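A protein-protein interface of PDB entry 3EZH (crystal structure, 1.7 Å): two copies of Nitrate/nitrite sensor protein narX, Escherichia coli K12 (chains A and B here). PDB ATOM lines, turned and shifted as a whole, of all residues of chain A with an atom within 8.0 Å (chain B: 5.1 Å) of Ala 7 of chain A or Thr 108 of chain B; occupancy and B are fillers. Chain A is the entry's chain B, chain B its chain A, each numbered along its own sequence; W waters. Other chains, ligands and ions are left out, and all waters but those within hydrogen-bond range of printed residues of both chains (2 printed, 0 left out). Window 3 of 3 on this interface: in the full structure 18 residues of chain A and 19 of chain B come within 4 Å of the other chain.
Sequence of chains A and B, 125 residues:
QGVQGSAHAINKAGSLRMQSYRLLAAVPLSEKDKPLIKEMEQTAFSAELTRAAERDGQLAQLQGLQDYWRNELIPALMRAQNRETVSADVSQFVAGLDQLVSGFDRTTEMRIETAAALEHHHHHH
Ile 10 of chain A touches its own counterpart, Ile 10 of chain B.
Of the 10 pairs that touch across the chains among the printed residues, 1 has its exchanged pair printed and touching as well.
Of chain B, only Ile 10, Asp 105, Thr 108 and Glu 109 come within 4 Å of Ala 7 of chain A.
Printed residues of chain B within 4 Å of His 8 of chain A: Asp 105.
Of the printed residues of chain B, Ser 6 of chain A touches Glu 109.
The nearest printed residue of chain A that does not touch Glu 109 of chain B is His 8 of chain A (4.6 Å).
Water W2 lies within hydrogen-bond range of the side-chain carboxylate (OE1) of Glu 109 of chain B, the backbone NH (N) of His 8 of chain A and the backbone NH (N) of Gly 5 of chain A.
Water W1 lies within hydrogen-bond range of O of Ile 10 of chain A (3.0 Å) and O of Ile 10 of chain B (3.2 Å).
Gly 5 of chain A touches Glu 109 of chain B (CA to OE1, 3.7 Å).
N of Ser 6 of chain A touches OE1 of Glu 109 of chain B, 3.5 Å away.
Ala 7 of chain A touches Ile 10 of chain B.
Ala 7 of chain A touches Thr 108 of chain B.
Glu 109 of chain B touches Ala 7 of chain A (OE1 to N, 3.5 Å).
CG2 of Ile 10 of chain B touches CG2 of Ile 10 of chain A, at 3.9 Å.
Asn 11 of chain A touches Ile 10 of chain B.
The backbone carbonyl oxygen (O) of Phe 104 of chain B is in hydrogen-bond range of the side-chain hydroxyl (OG1) of Thr 108 of chain B, 2.6 Å away.
The side-chain hydroxyl (OG) of Ser 6 of chain A lies close to the side-chain hydroxyl (OG1) of Thr 108 of chain A.
The side-chain carboxylate of Asp 105 of chain B lies within hydrogen-bond range of a ring nitrogen (ND1) of His 8 of chain A, at 3.4 Å.
ND2 of Asn 11 of chain A is in hydrogen-bond range of OD1 of Asp 105 of chain B, 2.9 Å away.
The side-chain carboxylate of Asp 105 of chain B sits close to the backbone carbonyl oxygen of Ala 7 of chain A, 3.5 Å away.
Hydrophobic or aromatic side chains of chain B within 4 Å of the printed part of chain A: Ile 10.
Along chain B the printed residues that touch a printed residue of chain A span positions 10 to 109.
Printed residues of chain A that touch a printed residue of chain B: Gly 5, Ser 6, Ala 7, His 8, Ile 10 and Asn 11.
Hydrophobic or aromatic side chains of chain A that line the printed part of chain B: Ala 7, His 8 and Ile 10.
Along chain A the printed residues that touch a printed residue of chain B span positions 5 to 11.
Among the printed residues, no Asp or Glu carboxylate lies within 4 Å of a Lys or Arg side-chain nitrogen of the other chain.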
ATOM      1  N   GLY A   5       8.107  22.439 -11.403  1.00  0.00           N
ATOM      2  CA  GLY A   5       8.476  21.212 -12.174  1.00  0.00           C
ATOM      3  C   GLY A   5       9.253  20.195 -11.364  1.00  0.00           C
ATOM      4  O   GLY A   5       9.326  20.284 -10.136  1.00  0.00           O
ATOM      5  N   SER A   6       9.853  19.234 -12.053  1.00  0.00           N
ATOM      6  CA  SER A   6      10.624  18.178 -11.414  1.00  0.00           C
ATOM      7  C   SER A   6      11.981  18.653 -10.911  1.00  0.00           C
ATOM      8  O   SER A   6      12.384  18.315  -9.800  1.00  0.00           O
ATOM      9  CB  SER A   6      10.872  17.043 -12.391  1.00  0.00           C
ATOM     10  OG  SER A   6      12.165  17.165 -12.970  1.00  0.00           O
ATOM     11  N   ALA A   7      12.693  19.404 -11.748  1.00  0.00           N
ATOM     12  CA  ALA A   7      14.022  19.913 -11.392  1.00  0.00           C
ATOM     13  C   ALA A   7      13.921  20.752 -10.124  1.00  0.00           C
ATOM     14  O   ALA A   7      14.781  20.689  -9.240  1.00  0.00           O
ATOM     15  CB  ALA A   7      14.580  20.749 -12.541  1.00  0.00           C
ATOM     16  N   HIS A   8      12.854  21.530 -10.025  1.00  0.00           N
ATOM     17  CA  HIS A   8      12.630  22.358  -8.857  1.00  0.00           C
ATOM     18  C   HIS A   8      12.316  21.522  -7.604  1.00  0.00           C
ATOM     19  O   HIS A   8      12.724  21.861  -6.499  1.00  0.00           O
ATOM     20  CB  HIS A   8      11.512  23.314  -9.141  1.00  0.00           C
ATOM     21  CG  HIS A   8      11.239  24.266  -8.023  1.00  0.00           C
ATOM     22  ND1 HIS A   8      12.141  25.232  -7.626  1.00  0.00           N
ATOM     23  CD2 HIS A   8      10.163  24.407  -7.218  1.00  0.00           C
ATOM     24  CE1 HIS A   8      11.630  25.925  -6.624  1.00  0.00           C
ATOM     25  NE2 HIS A   8      10.430  25.444  -6.359  1.00  0.00           N
ATOM     26  N   ALA A   9      11.555  20.446  -7.769  1.00  0.00           N
ATOM     27  CA  ALA A   9      11.244  19.584  -6.622  1.00  0.00           C
ATOM     28  C   ALA A   9      12.523  18.873  -6.116  1.00  0.00           C
ATOM     29  O   ALA A   9      12.668  18.614  -4.932  1.00  0.00           O
ATOM     30  CB  ALA A   9      10.160  18.525  -7.055  1.00  0.00           C
ATOM     31  N   ILE A  10      13.460  18.545  -7.007  1.00  0.00           N
ATOM     32  CA  ILE A  10      14.704  17.888  -6.594  1.00  0.00           C
ATOM     33  C   ILE A  10      15.506  18.920  -5.741  1.00  0.00           C
ATOM     34  O   ILE A  10      16.134  18.565  -4.752  1.00  0.00           O
ATOM     35  CB  ILE A  10      15.546  17.469  -7.807  1.00  0.00           C
ATOM     36  CG1 ILE A  10      14.779  16.387  -8.583  1.00  0.00           C
ATOM     37  CG2 ILE A  10      16.943  17.040  -7.390  1.00  0.00           C
ATOM     38  CD1 ILE A  10      15.482  16.005  -9.864  1.00  0.00           C
ATOM     39  N   ASN A  11      15.435  20.190  -6.133  1.00  0.00           N
ATOM     40  CA  ASN A  11      16.123  21.279  -5.381  1.00  0.00           C
ATOM     41  C   ASN A  11      15.485  21.446  -3.998  1.00  0.00           C
ATOM     42  O   ASN A  11      16.157  21.429  -2.977  1.00  0.00           O
ATOM     43  CB  ASN A  11      15.991  22.613  -6.187  1.00  0.00           C
ATOM     44  CG  ASN A  11      16.645  23.807  -5.487  1.00  0.00           C
ATOM     45  OD1 ASN A  11      17.239  23.662  -4.425  1.00  0.00           O
ATOM     46  ND2 ASN A  11      16.514  25.009  -6.084  1.00  0.00           N
ATOM     47  N   LYS A  12      14.159  21.547  -3.963  1.00  0.00           N
ATOM     48  CA  LYS A  12      13.428  21.781  -2.718  1.00  0.00           C
ATOM     49  C   LYS A  12      13.490  20.601  -1.738  1.00  0.00           C
ATOM     50  O   LYS A  12      13.739  20.761  -0.548  1.00  0.00           O
ATOM     51  CB  LYS A  12      11.998  22.143  -3.078  1.00  0.00           C
ATOM     52  CG  LYS A  12      11.829  23.571  -3.503  1.00  0.00           C
ATOM     53  CD  LYS A  12      12.203  24.491  -2.367  1.00  0.00           C
ATOM     54  CE  LYS A  12      13.057  25.645  -2.860  1.00  0.00           C
ATOM     55  NZ  LYS A  12      13.496  26.483  -1.701  1.00  0.00           N
ATOM     56  N   ALA A  13      13.309  19.385  -2.258  1.00  0.00           N
ATOM     57  CA  ALA A  13      13.435  18.195  -1.375  1.00  0.00           C
ATOM     58  C   ALA A  13      14.885  18.112  -0.882  1.00  0.00           C
ATOM     59  O   ALA A  13      15.166  17.820   0.275  1.00  0.00           O
ATOM     60  CB  ALA A  13      13.101  16.903  -2.181  1.00  0.00           C
ATOM     61  N   GLY A  14      15.824  18.382  -1.787  1.00  0.00           N
ATOM     62  CA  GLY A  14      17.221  18.337  -1.403  1.00  0.00           C
ATOM     63  C   GLY A  14      17.472  19.340  -0.284  1.00  0.00           C
ATOM     64  O   GLY A  14      18.236  19.078   0.619  1.00  0.00           O
ATOM     65  N   ALA A  52       4.822  16.694  -6.487  1.00  0.00           N
ATOM     66  CA  ALA A  52       5.915  15.988  -7.102  1.00  0.00           C
ATOM     67  C   ALA A  52       6.006  14.564  -6.586  1.00  0.00           C
ATOM     68  O   ALA A  52       6.282  13.651  -7.352  1.00  0.00           O
ATOM     69  CB  ALA A  52       7.256  16.715  -6.861  1.00  0.00           C
ATOM     70  N   ASP A  56       5.570  11.134  -8.812  1.00  0.00           N
ATOM     71  CA  ASP A  56       6.699  10.211  -8.912  1.00  0.00           C
ATOM     72  C   ASP A  56       6.610   8.914  -8.136  1.00  0.00           C
ATOM     73  O   ASP A  56       7.548   8.104  -8.159  1.00  0.00           O
ATOM     74  CB  ASP A  56       7.965  10.967  -8.515  1.00  0.00           C
ATOM     75  CG  ASP A  56       8.213  12.190  -9.388  1.00  0.00           C
ATOM     76  OD1 ASP A  56       8.967  13.090  -8.958  1.00  0.00           O
ATOM     77  OD2 ASP A  56       7.675  12.273 -10.505  1.00  0.00           O
ATOM     78  N   PHE A 104      12.946  11.219  -6.895  1.00  0.00           N
ATOM     79  CA  PHE A 104      12.565  12.350  -7.782  1.00  0.00           C
ATOM     80  C   PHE A 104      13.524  12.446  -8.955  1.00  0.00           C
ATOM     81  O   PHE A 104      13.132  12.615 -10.141  1.00  0.00           O
ATOM     82  CB  PHE A 104      12.646  13.699  -7.037  1.00  0.00           C
ATOM     83  CG  PHE A 104      11.561  13.932  -6.053  1.00  0.00           C
ATOM     84  CD1 PHE A 104      10.594  12.966  -5.791  1.00  0.00           C
ATOM     85  CD2 PHE A 104      11.489  15.131  -5.389  1.00  0.00           C
ATOM     86  CE1 PHE A 104       9.568  13.224  -4.870  1.00  0.00           C
ATOM     87  CE2 PHE A 104      10.472  15.386  -4.480  1.00  0.00           C
ATOM     88  CZ  PHE A 104       9.514  14.439  -4.225  1.00  0.00           C
ATOM     89  N   ASP A 105      14.794  12.350  -8.622  1.00  0.00           N
ATOM     90  CA  ASP A 105      15.867  12.443  -9.584  1.00  0.00           C
ATOM     91  C   ASP A 105      15.740  11.285 -10.610  1.00  0.00           C
ATOM     92  O   ASP A 105      15.599  11.545 -11.830  1.00  0.00           O
ATOM     93  CB  ASP A 105      17.173  12.596  -8.720  1.00  0.00           C
ATOM     94  CG  ASP A 105      18.419  12.005  -9.309  1.00  0.00           C
ATOM     95  OD1 ASP A 105      19.477  12.131  -8.617  1.00  0.00           O
ATOM     96  OD2 ASP A 105      18.381  11.418 -10.413  1.00  0.00           O
ATOM     97  N   THR A 108      12.564  11.494 -12.780  1.00  0.00           N
ATOM     98  CA  THR A 108      12.624  12.587 -13.716  1.00  0.00           C
ATOM     99  C   THR A 108      13.473  12.168 -14.903  1.00  0.00           C
ATOM    100  O   THR A 108      13.105  12.415 -16.066  1.00  0.00           O
ATOM    101  CB  THR A 108      13.180  13.834 -13.062  1.00  0.00           C
ATOM    102  OG1 THR A 108      12.190  14.372 -12.179  1.00  0.00           O
ATOM    103  CG2 THR A 108      13.473  14.883 -14.102  1.00  0.00           C
ATOM    104  N   ILE A 112      12.745  11.498 -18.959  1.00  0.00           N
ATOM    105  CA  ILE A 112      13.619  12.044 -20.015  1.00  0.00           C
ATOM    106  C   ILE A 112      13.912  10.987 -21.065  1.00  0.00           C
ATOM    107  O   ILE A 112      13.705  11.190 -22.267  1.00  0.00           O
ATOM    108  CB  ILE A 112      14.998  12.477 -19.452  1.00  0.00           C
ATOM    109  CG1 ILE A 112      14.863  13.750 -18.631  1.00  0.00           C
ATOM    110  CG2 ILE A 112      16.007  12.656 -20.602  1.00  0.00           C
ATOM    111  CD1 ILE A 112      16.199  14.310 -18.176  1.00  0.00           C
ATOM    112  N   SER B   6      20.697  15.914 -16.311  1.00  0.00           N
ATOM    113  CA  SER B   6      20.367  17.174 -15.664  1.00  0.00           C
ATOM    114  C   SER B   6      19.834  17.001 -14.259  1.00  0.00           C
ATOM    115  O   SER B   6      20.199  17.766 -13.366  1.00  0.00           O
ATOM    116  CB  SER B   6      19.353  17.967 -16.488  1.00  0.00           C
ATOM    117  OG  SER B   6      19.933  18.456 -17.674  1.00  0.00           O
ATOM    118  N   ILE B  10      21.382  18.358 -10.359  1.00  0.00           N
ATOM    119  CA  ILE B  10      20.701  19.274  -9.391  1.00  0.00           C
ATOM    120  C   ILE B  10      20.826  18.616  -8.000  1.00  0.00           C
ATOM    121  O   ILE B  10      21.114  19.267  -7.024  1.00  0.00           O
ATOM    122  CB  ILE B  10      19.221  19.509  -9.759  1.00  0.00           C
ATOM    123  CG1 ILE B  10      19.173  20.222 -11.111  1.00  0.00           C
ATOM    124  CG2 ILE B  10      18.437  20.393  -8.730  1.00  0.00           C
ATOM    125  CD1 ILE B  10      17.780  20.513 -11.592  1.00  0.00           C
ATOM    126  N   ASP B  56      24.122  25.237 -18.250  1.00  0.00           N
ATOM    127  CA  ASP B  56      23.163  26.176 -17.662  1.00  0.00           C
ATOM    128  C   ASP B  56      23.579  27.632 -17.528  1.00  0.00           C
ATOM    129  O   ASP B  56      22.819  28.448 -16.959  1.00  0.00           O
ATOM    130  CB  ASP B  56      22.650  25.632 -16.306  1.00  0.00           C
ATOM    131  CG  ASP B  56      22.138  24.173 -16.418  1.00  0.00           C
ATOM    132  OD1 ASP B  56      21.551  23.822 -17.467  1.00  0.00           O
ATOM    133  OD2 ASP B  56      22.317  23.367 -15.467  1.00  0.00           O
ATOM    134  N   GLY B 103      19.863  28.458 -10.522  1.00  0.00           N
ATOM    135  CA  GLY B 103      20.251  28.737 -11.901  1.00  0.00           C
ATOM    136  C   GLY B 103      20.133  27.453 -12.698  1.00  0.00           C
ATOM    137  O   GLY B 103      19.617  27.474 -13.834  1.00  0.00           O
ATOM    138  N   PHE B 104      20.629  26.346 -12.140  1.00  0.00           N
ATOM    139  CA  PHE B 104      20.524  25.028 -12.782  1.00  0.00           C
ATOM    140  C   PHE B 104      19.012  24.739 -12.993  1.00  0.00           C
ATOM    141  O   PHE B 104      18.607  24.122 -13.995  1.00  0.00           O
ATOM    142  CB  PHE B 104      21.082  23.922 -11.900  1.00  0.00           C
ATOM    143  CG  PHE B 104      22.600  23.780 -11.900  1.00  0.00           C
ATOM    144  CD1 PHE B 104      23.444  24.806 -12.326  1.00  0.00           C
ATOM    145  CD2 PHE B 104      23.187  22.632 -11.381  1.00  0.00           C
ATOM    146  CE1 PHE B 104      24.829  24.662 -12.209  1.00  0.00           C
ATOM    147  CE2 PHE B 104      24.568  22.487 -11.269  1.00  0.00           C
ATOM    148  CZ  PHE B 104      25.409  23.519 -11.690  1.00  0.00           C
ATOM    149  N   ASP B 105      18.181  25.181 -12.048  1.00  0.00           N
ATOM    150  CA  ASP B 105      16.734  24.974 -12.154  1.00  0.00           C
ATOM    151  C   ASP B 105      16.088  25.625 -13.336  1.00  0.00           C
ATOM    152  O   ASP B 105      15.407  24.961 -14.093  1.00  0.00           O
ATOM    153  CB  ASP B 105      15.970  25.510 -10.932  1.00  0.00           C
ATOM    154  CG  ASP B 105      15.974  24.561  -9.764  1.00  0.00           C
ATOM    155  OD1 ASP B 105      15.308  24.865  -8.752  1.00  0.00           O
ATOM    156  OD2 ASP B 105      16.664  23.543  -9.859  1.00  0.00           O
ATOM    157  N   ARG B 106      16.252  26.943 -13.468  1.00  0.00           N
ATOM    158  CA  ARG B 106      15.587  27.647 -14.544  1.00  0.00           C
ATOM    159  C   ARG B 106      15.889  27.007 -15.867  1.00  0.00           C
ATOM    160  O   ARG B 106      14.981  26.612 -16.605  1.00  0.00           O
ATOM    161  CB  ARG B 106      15.992  29.133 -14.646  1.00  0.00           C
ATOM    162  CG  ARG B 106      15.193  29.830 -15.741  1.00  0.00           C
ATOM    163  CD  ARG B 106      15.355  31.324 -15.688  1.00  0.00           C
ATOM    164  NE  ARG B 106      16.748  31.665 -15.911  1.00  0.00           N
ATOM    165  CZ  ARG B 106      17.321  31.660 -17.112  1.00  0.00           C
ATOM    166  NH1 ARG B 106      16.600  31.335 -18.185  1.00  0.00           N
ATOM    167  NH2 ARG B 106      18.609  31.988 -17.232  1.00  0.00           N
ATOM    168  N   THR B 107      17.181  26.905 -16.152  1.00  0.00           N
ATOM    169  CA  THR B 107      17.663  26.366 -17.413  1.00  0.00           C
ATOM    170  C   THR B 107      17.253  24.938 -17.631  1.00  0.00           C
ATOM    171  O   THR B 107      16.759  24.585 -18.710  1.00  0.00           O
ATOM    172  CB  THR B 107      19.190  26.523 -17.469  1.00  0.00           C
ATOM    173  OG1 THR B 107      19.478  27.914 -17.252  1.00  0.00           O
ATOM    174  CG2 THR B 107      19.749  26.109 -18.816  1.00  0.00           C
ATOM    175  N   THR B 108      17.418  24.118 -16.614  1.00  0.00           N
ATOM    176  CA  THR B 108      17.039  22.709 -16.735  1.00  0.00           C
ATOM    177  C   THR B 108      15.560  22.460 -16.990  1.00  0.00           C
ATOM    178  O   THR B 108      15.188  21.621 -17.834  1.00  0.00           O
ATOM    179  CB  THR B 108      17.419  21.902 -15.485  1.00  0.00           C
ATOM    180  OG1 THR B 108      18.844  21.887 -15.341  1.00  0.00           O
ATOM    181  CG2 THR B 108      16.919  20.458 -15.608  1.00  0.00           C
ATOM    182  N   GLU B 109      14.705  23.154 -16.250  1.00  0.00           N
ATOM    183  CA  GLU B 109      13.271  22.928 -16.428  1.00  0.00           C
ATOM    184  C   GLU B 109      12.935  23.255 -17.880  1.00  0.00           C
ATOM    185  O   GLU B 109      12.224  22.495 -18.555  1.00  0.00           O
ATOM    186  CB  GLU B 109      12.438  23.809 -15.501  1.00  0.00           C
ATOM    187  CG  GLU B 109      10.941  23.422 -15.504  1.00  0.00           C
ATOM    188  CD  GLU B 109      10.692  21.931 -15.200  1.00  0.00           C
ATOM    189  OE1 GLU B 109      11.440  21.331 -14.390  1.00  0.00           O
ATOM    190  OE2 GLU B 109       9.724  21.361 -15.770  1.00  0.00           O
ATOM    191  N   MET B 110      13.483  24.364 -18.355  1.00  0.00           N
ATOM    192  CA  MET B 110      13.246  24.804 -19.721  1.00  0.00           C
ATOM    193  C   MET B 110      13.667  23.787 -20.776  1.00  0.00           C
ATOM    194  O   MET B 110      12.910  23.489 -21.704  1.00  0.00           O
ATOM    195  CB  MET B 110      13.995  26.098 -19.961  1.00  0.00           C
ATOM    196  CG  MET B 110      13.396  26.944 -21.039  1.00  0.00           C
ATOM    197  SD  MET B 110      13.602  28.764 -20.499  1.00  0.00           S
ATOM    198  CE  MET B 110      12.800  28.631 -18.744  1.00  0.00           C
ATOM    199  N   ARG B 111      14.883  23.273 -20.640  1.00  0.00           N
ATOM    200  CA  ARG B 111      15.415  22.308 -21.584  1.00  0.00           C
ATOM    201  C   ARG B 111      14.534  21.068 -21.653  1.00  0.00           C
ATOM    202  O   ARG B 111      14.387  20.450 -22.725  1.00  0.00           O
ATOM    203  CB  ARG B 111      16.856  21.919 -21.220  1.00  0.00           C
ATOM    204  CG  ARG B 111      17.914  22.967 -21.584  1.00  0.00           C
ATOM    205  CD  ARG B 111      19.103  22.879 -20.621  1.00  0.00           C
ATOM    206  NE  ARG B 111      19.892  21.674 -20.849  1.00  0.00           N
ATOM    207  CZ  ARG B 111      20.660  21.084 -19.933  1.00  0.00           C
ATOM    208  NH1 ARG B 111      20.752  21.577 -18.693  1.00  0.00           N
ATOM    209  NH2 ARG B 111      21.345  19.987 -20.267  1.00  0.00           N
ATOM    210  N   ILE B 112      13.923  20.711 -20.527  1.00  0.00           N
ATOM    211  CA  ILE B 112      13.061  19.540 -20.499  1.00  0.00           C
ATOM    212  C   ILE B 112      11.700  19.813 -21.162  1.00  0.00           C
ATOM    213  O   ILE B 112      11.227  19.039 -21.991  1.00  0.00           O
ATOM    214  CB  ILE B 112      12.904  19.040 -19.014  1.00  0.00           C
ATOM    215  CG1 ILE B 112      14.193  18.327 -18.591  1.00  0.00           C
ATOM    216  CG2 ILE B 112      11.679  18.124 -18.890  1.00  0.00           C
ATOM    217  CD1 ILE B 112      14.514  18.342 -17.076  1.00  0.00           C
HETATM  218  O   HOH W   1      19.127  19.028  -4.465  1.00  0.00           O
HETATM  219  O   HOH W   2      11.234  23.036 -12.278  1.00  0.00           O
